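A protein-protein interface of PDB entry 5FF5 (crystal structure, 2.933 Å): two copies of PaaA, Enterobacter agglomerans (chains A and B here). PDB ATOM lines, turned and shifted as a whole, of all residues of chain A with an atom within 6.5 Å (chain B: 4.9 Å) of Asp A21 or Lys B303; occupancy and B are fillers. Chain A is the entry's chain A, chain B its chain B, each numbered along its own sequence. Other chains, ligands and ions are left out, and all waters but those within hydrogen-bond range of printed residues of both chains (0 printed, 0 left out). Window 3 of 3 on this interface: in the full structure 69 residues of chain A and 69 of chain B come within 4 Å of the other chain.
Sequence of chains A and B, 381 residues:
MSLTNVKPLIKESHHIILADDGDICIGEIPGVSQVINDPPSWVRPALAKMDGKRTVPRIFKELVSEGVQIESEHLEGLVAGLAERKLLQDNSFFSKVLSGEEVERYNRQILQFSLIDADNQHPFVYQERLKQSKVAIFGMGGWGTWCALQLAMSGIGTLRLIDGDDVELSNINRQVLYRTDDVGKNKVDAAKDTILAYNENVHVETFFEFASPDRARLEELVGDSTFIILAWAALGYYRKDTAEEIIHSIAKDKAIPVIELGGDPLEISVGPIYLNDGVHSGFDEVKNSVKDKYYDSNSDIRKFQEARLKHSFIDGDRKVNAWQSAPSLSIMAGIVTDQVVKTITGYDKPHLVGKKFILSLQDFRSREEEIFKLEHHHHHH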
ATOM      1  N   ILE A  17      32.615  18.145   6.933  1.00  0.00           N
ATOM      2  CA  ILE A  17      32.618  17.495   8.235  1.00  0.00           C
ATOM      3  C   ILE A  17      32.939  15.997   8.147  1.00  0.00           C
ATOM      4  O   ILE A  17      32.564  15.325   7.179  1.00  0.00           O
ATOM      5  CB  ILE A  17      31.270  17.692   8.926  1.00  0.00           C
ATOM      6  CG1 ILE A  17      30.868  19.158   8.863  1.00  0.00           C
ATOM      7  CG2 ILE A  17      31.340  17.267  10.374  1.00  0.00           C
ATOM      8  CD1 ILE A  17      29.910  19.544   9.950  1.00  0.00           C
ATOM      9  N   LEU A  18      33.649  15.490   9.159  1.00  0.00           N
ATOM     10  CA  LEU A  18      34.044  14.080   9.218  1.00  0.00           C
ATOM     11  C   LEU A  18      33.417  13.354  10.407  1.00  0.00           C
ATOM     12  O   LEU A  18      33.892  13.453  11.548  1.00  0.00           O
ATOM     13  CB  LEU A  18      35.557  13.965   9.291  1.00  0.00           C
ATOM     14  CG  LEU A  18      36.109  12.602   8.919  1.00  0.00           C
ATOM     15  CD1 LEU A  18      35.421  12.086   7.677  1.00  0.00           C
ATOM     16  CD2 LEU A  18      37.588  12.738   8.672  1.00  0.00           C
ATOM     17  N   ALA A  19      32.339  12.630  10.139  1.00  0.00           N
ATOM     18  CA  ALA A  19      31.645  11.917  11.195  1.00  0.00           C
ATOM     19  C   ALA A  19      32.531  10.792  11.698  1.00  0.00           C
ATOM     20  O   ALA A  19      33.411  10.302  10.973  1.00  0.00           O
ATOM     21  CB  ALA A  19      30.333  11.383  10.702  1.00  0.00           C
ATOM     22  N   ASP A  20      32.304  10.382  12.939  1.00  0.00           N
ATOM     23  CA  ASP A  20      33.171   9.397  13.571  1.00  0.00           C
ATOM     24  C   ASP A  20      33.230   8.116  12.750  1.00  0.00           C
ATOM     25  O   ASP A  20      34.298   7.532  12.583  1.00  0.00           O
ATOM     26  CB  ASP A  20      32.699   9.124  14.998  1.00  0.00           C
ATOM     27  CG  ASP A  20      32.894  10.344  15.936  1.00  0.00           C
ATOM     28  OD1 ASP A  20      33.232  11.473  15.459  1.00  0.00           O
ATOM     29  OD2 ASP A  20      32.694  10.167  17.164  1.00  0.00           O
ATOM     30  N   ASP A  21      32.099   7.700  12.197  1.00  0.00           N
ATOM     31  CA  ASP A  21      32.077   6.493  11.371  1.00  0.00           C
ATOM     32  C   ASP A  21      32.661   6.698   9.958  1.00  0.00           C
ATOM     33  O   ASP A  21      32.693   5.762   9.154  1.00  0.00           O
ATOM     34  CB  ASP A  21      30.644   5.939  11.276  1.00  0.00           C
ATOM     35  CG  ASP A  21      29.649   6.930  10.645  1.00  0.00           C
ATOM     36  OD1 ASP A  21      30.075   7.866   9.919  1.00  0.00           O
ATOM     37  OD2 ASP A  21      28.421   6.752  10.862  1.00  0.00           O
ATOM     38  N   GLY A  22      33.113   7.911   9.646  1.00  0.00           N
ATOM     39  CA  GLY A  22      33.740   8.176   8.359  1.00  0.00           C
ATOM     40  C   GLY A  22      32.889   8.820   7.270  1.00  0.00           C
ATOM     41  O   GLY A  22      33.413   9.161   6.207  1.00  0.00           O
ATOM     42  N   ASP A  23      31.587   8.985   7.507  1.00  0.00           N
ATOM     43  CA  ASP A  23      30.710   9.649   6.536  1.00  0.00           C
ATOM     44  C   ASP A  23      31.067  11.126   6.441  1.00  0.00           C
ATOM     45  O   ASP A  23      31.594  11.693   7.395  1.00  0.00           O
ATOM     46  CB  ASP A  23      29.233   9.489   6.917  1.00  0.00           C
ATOM     47  CG  ASP A  23      28.774   8.037   6.895  1.00  0.00           C
ATOM     48  OD1 ASP A  23      29.446   7.219   6.237  1.00  0.00           O
ATOM     49  OD2 ASP A  23      27.745   7.702   7.527  1.00  0.00           O
ATOM     50  N   ILE A  24      30.787  11.748   5.298  1.00  0.00           N
ATOM     51  CA  ILE A  24      31.069  13.176   5.128  1.00  0.00           C
ATOM     52  C   ILE A  24      29.818  14.000   4.832  1.00  0.00           C
ATOM     53  O   ILE A  24      28.928  13.578   4.094  1.00  0.00           O
ATOM     54  CB  ILE A  24      32.072  13.435   4.000  1.00  0.00           C
ATOM     55  CG1 ILE A  24      31.507  12.902   2.674  1.00  0.00           C
ATOM     56  CG2 ILE A  24      33.428  12.815   4.329  1.00  0.00           C
ATOM     57  CD1 ILE A  24      31.947  13.689   1.440  1.00  0.00           C
ATOM     58  N   VAL A  35      25.124  14.837   1.771  1.00  0.00           N
ATOM     59  CA  VAL A  35      25.675  13.867   2.691  1.00  0.00           C
ATOM     60  C   VAL A  35      26.148  12.666   1.890  1.00  0.00           C
ATOM     61  O   VAL A  35      25.335  11.915   1.351  1.00  0.00           O
ATOM     62  CB  VAL A  35      24.641  13.422   3.741  1.00  0.00           C
ATOM     63  CG1 VAL A  35      25.172  12.248   4.522  1.00  0.00           C
ATOM     64  CG2 VAL A  35      24.297  14.574   4.664  1.00  0.00           C
ATOM     65  N   ASN A  37      27.462   9.134   2.001  1.00  0.00           N
ATOM     66  CA  ASN A  37      27.565   7.978   2.890  1.00  0.00           C
ATOM     67  C   ASN A  37      28.639   7.011   2.411  1.00  0.00           C
ATOM     68  O   ASN A  37      28.789   6.789   1.214  1.00  0.00           O
ATOM     69  CB  ASN A  37      26.230   7.228   2.996  1.00  0.00           C
ATOM     70  CG  ASN A  37      25.069   8.135   3.341  1.00  0.00           C
ATOM     71  OD1 ASN A  37      24.921   8.571   4.485  1.00  0.00           O
ATOM     72  ND2 ASN A  37      24.224   8.413   2.353  1.00  0.00           N
ATOM     73  N   SER B 299      21.987   9.315   7.064  1.00  0.00           N
ATOM     74  CA  SER B 299      22.542  10.571   7.586  1.00  0.00           C
ATOM     75  C   SER B 299      21.854  11.071   8.873  1.00  0.00           C
ATOM     76  O   SER B 299      20.700  11.511   8.850  1.00  0.00           O
ATOM     77  CB  SER B 299      22.462  11.664   6.516  1.00  0.00           C
ATOM     78  N   ASP B 300      22.572  11.004   9.992  1.00  0.00           N
ATOM     79  CA  ASP B 300      22.066  11.516  11.262  1.00  0.00           C
ATOM     80  C   ASP B 300      22.217  13.043  11.314  1.00  0.00           C
ATOM     81  O   ASP B 300      23.323  13.570  11.164  1.00  0.00           O
ATOM     82  CB  ASP B 300      22.801  10.861  12.453  1.00  0.00           C
ATOM     83  CG  ASP B 300      22.153   9.549  12.906  1.00  0.00           C
ATOM     84  OD1 ASP B 300      20.911   9.478  12.999  1.00  0.00           O
ATOM     85  OD2 ASP B 300      22.887   8.576  13.179  1.00  0.00           O
ATOM     86  N   ILE B 301      21.115  13.757  11.522  1.00  0.00           N
ATOM     87  CA  ILE B 301      21.221  15.173  11.840  1.00  0.00           C
ATOM     88  C   ILE B 301      22.036  15.351  13.130  1.00  0.00           C
ATOM     89  O   ILE B 301      22.485  16.459  13.434  1.00  0.00           O
ATOM     90  CB  ILE B 301      19.838  15.836  12.012  1.00  0.00           C
ATOM     91  N   ARG B 302      22.235  14.255  13.870  1.00  0.00           N
ATOM     92  CA  ARG B 302      22.877  14.309  15.184  1.00  0.00           C
ATOM     93  C   ARG B 302      24.375  14.101  15.112  1.00  0.00           C
ATOM     94  O   ARG B 302      25.134  14.820  15.762  1.00  0.00           O
ATOM     95  CB  ARG B 302      22.278  13.266  16.132  1.00  0.00           C
ATOM     96  N   LYS B 303      24.802  13.114  14.330  1.00  0.00           N
ATOM     97  CA  LYS B 303      26.212  12.725  14.282  1.00  0.00           C
ATOM     98  C   LYS B 303      27.088  13.807  13.657  1.00  0.00           C
ATOM     99  O   LYS B 303      28.223  14.026  14.093  1.00  0.00           O
ATOM    100  CB  LYS B 303      26.371  11.423  13.516  1.00  0.00           C
ATOM    101  CG  LYS B 303      26.349  11.568  12.017  1.00  0.00           C
ATOM    102  CD  LYS B 303      26.381  10.198  11.385  1.00  0.00           C
ATOM    103  CE  LYS B 303      26.528  10.262   9.900  1.00  0.00           C
ATOM    104  NZ  LYS B 303      26.559   8.884   9.406  1.00  0.00           N
ATOM    105  N   PHE B 304      26.557  14.496  12.650  1.00  0.00           N
ATOM    106  CA  PHE B 304      27.270  15.624  12.078  1.00  0.00           C
ATOM    107  C   PHE B 304      27.188  16.835  12.993  1.00  0.00           C
ATOM    108  O   PHE B 304      28.077  17.689  12.978  1.00  0.00           O
ATOM    109  CB  PHE B 304      26.732  15.940  10.698  1.00  0.00           C
ATOM    110  CG  PHE B 304      27.095  14.911   9.671  1.00  0.00           C
ATOM    111  CD1 PHE B 304      28.403  14.805   9.216  1.00  0.00           C
ATOM    112  CD2 PHE B 304      26.139  14.042   9.167  1.00  0.00           C
ATOM    113  CE1 PHE B 304      28.753  13.851   8.273  1.00  0.00           C
ATOM    114  CE2 PHE B 304      26.480  13.087   8.219  1.00  0.00           C
ATOM    115  CZ  PHE B 304      27.793  12.986   7.774  1.00  0.00           C
ATOM    116  N   GLN B 305      26.141  16.896  13.811  1.00  0.00           N
ATOM    117  CA  GLN B 305      26.107  17.880  14.886  1.00  0.00           C
ATOM    118  C   GLN B 305      27.302  17.637  15.792  1.00  0.00           C
ATOM    119  O   GLN B 305      28.110  18.544  16.009  1.00  0.00           O
ATOM    120  CB  GLN B 305      24.798  17.812  15.689  1.00  0.00           C
ATOM    121  CG  GLN B 305      24.722  18.777  16.896  1.00  0.00           C
ATOM    122  CD  GLN B 305      24.595  20.270  16.508  1.00  0.00           C
ATOM    123  OE1 GLN B 305      24.527  20.619  15.321  1.00  0.00           O
ATOM    124  NE2 GLN B 305      24.560  21.149  17.522  1.00  0.00           N
ATOM    125  N   GLU B 306      27.417  16.398  16.285  1.00  0.00           N
ATOM    126  CA  GLU B 306      28.462  15.997  17.240  1.00  0.00           C
ATOM    127  C   GLU B 306      29.868  16.229  16.677  1.00  0.00           C
ATOM    128  O   GLU B 306      30.724  16.839  17.335  1.00  0.00           O
ATOM    129  CB  GLU B 306      28.301  14.523  17.643  1.00  0.00           C
ATOM    130  CG  GLU B 306      26.853  14.074  17.957  1.00  0.00           C
ATOM    131  CD  GLU B 306      26.297  14.594  19.294  1.00  0.00           C
ATOM    132  OE1 GLU B 306      26.968  14.415  20.336  1.00  0.00           O
ATOM    133  OE2 GLU B 306      25.178  15.172  19.304  1.00  0.00           O
ATOM    134  N   ALA B 307      30.091  15.750  15.454  1.00  0.00           N
ATOM    135  CA  ALA B 307      31.359  15.966  14.759  1.00  0.00           C
ATOM    136  C   ALA B 307      31.729  17.433  14.577  1.00  0.00           C
ATOM    137  O   ALA B 307      32.907  17.770  14.597  1.00  0.00           O
ATOM    138  CB  ALA B 307      31.327  15.296  13.425  1.00  0.00           C
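The side-chain amino group (NZ) of Lys B303 is in salt-bridge range of the side-chain carboxylate (OD2) of Asp A23.
OD2 of Asp A21 lies within salt-bridge range of NZ of Lys B303.
N of Asp A23 lies within hydrogen-bond range of OD1 of Asp A21.
O of Phe B304 touches CD1 of Ile A17, at 3.996 Å.
Ala B307 touches Ile A17 (CB to CG2, 3.6 Å).
O of Leu A18 touches CB of Ala B307, 3.7 Å away.
Ala A19 touches Phe B304.
Asp A23 touches Phe B304.
Ile A24 touches Phe B304 (C to CE1, 3.6 Å).
Val A35 touches Ser B299 (CG1 to CB, 3.4 Å).
Ser B299 touches Asn A37 (N to OD1, 3.98 Å).
Of the printed residues of chain B, Ala A19 touches Phe B304.
Asp A20 touches none of the printed residues of chain B.
Of chain B, only Lys B303 comes within 4 Å of Asp A21.
Of the printed residues of chain B, Ile A24 touches Phe B304 (3.6 Å).
Ile B301 touches none of the printed residues of chain A.
Lys B303 touches two residues of chain A.
Of the printed residues of chain A, Ala B307 touches Ile A17 (3.6 Å) and Leu A18 (3.7 Å).
The nearest printed residue of chain B that does not touch Asp A21 is Phe B304 (6.0 Å).
Of the 10 printed residues of chain A, 8 touch a printed residue of chain B.
Of the 9 printed residues of chain B, 4 touch a printed residue of chain A.
Printed residues of chain B that touch a printed residue of chain A: Ser B299, Lys B303, Phe B304 and Ala B307.
No position is printed for both chains.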
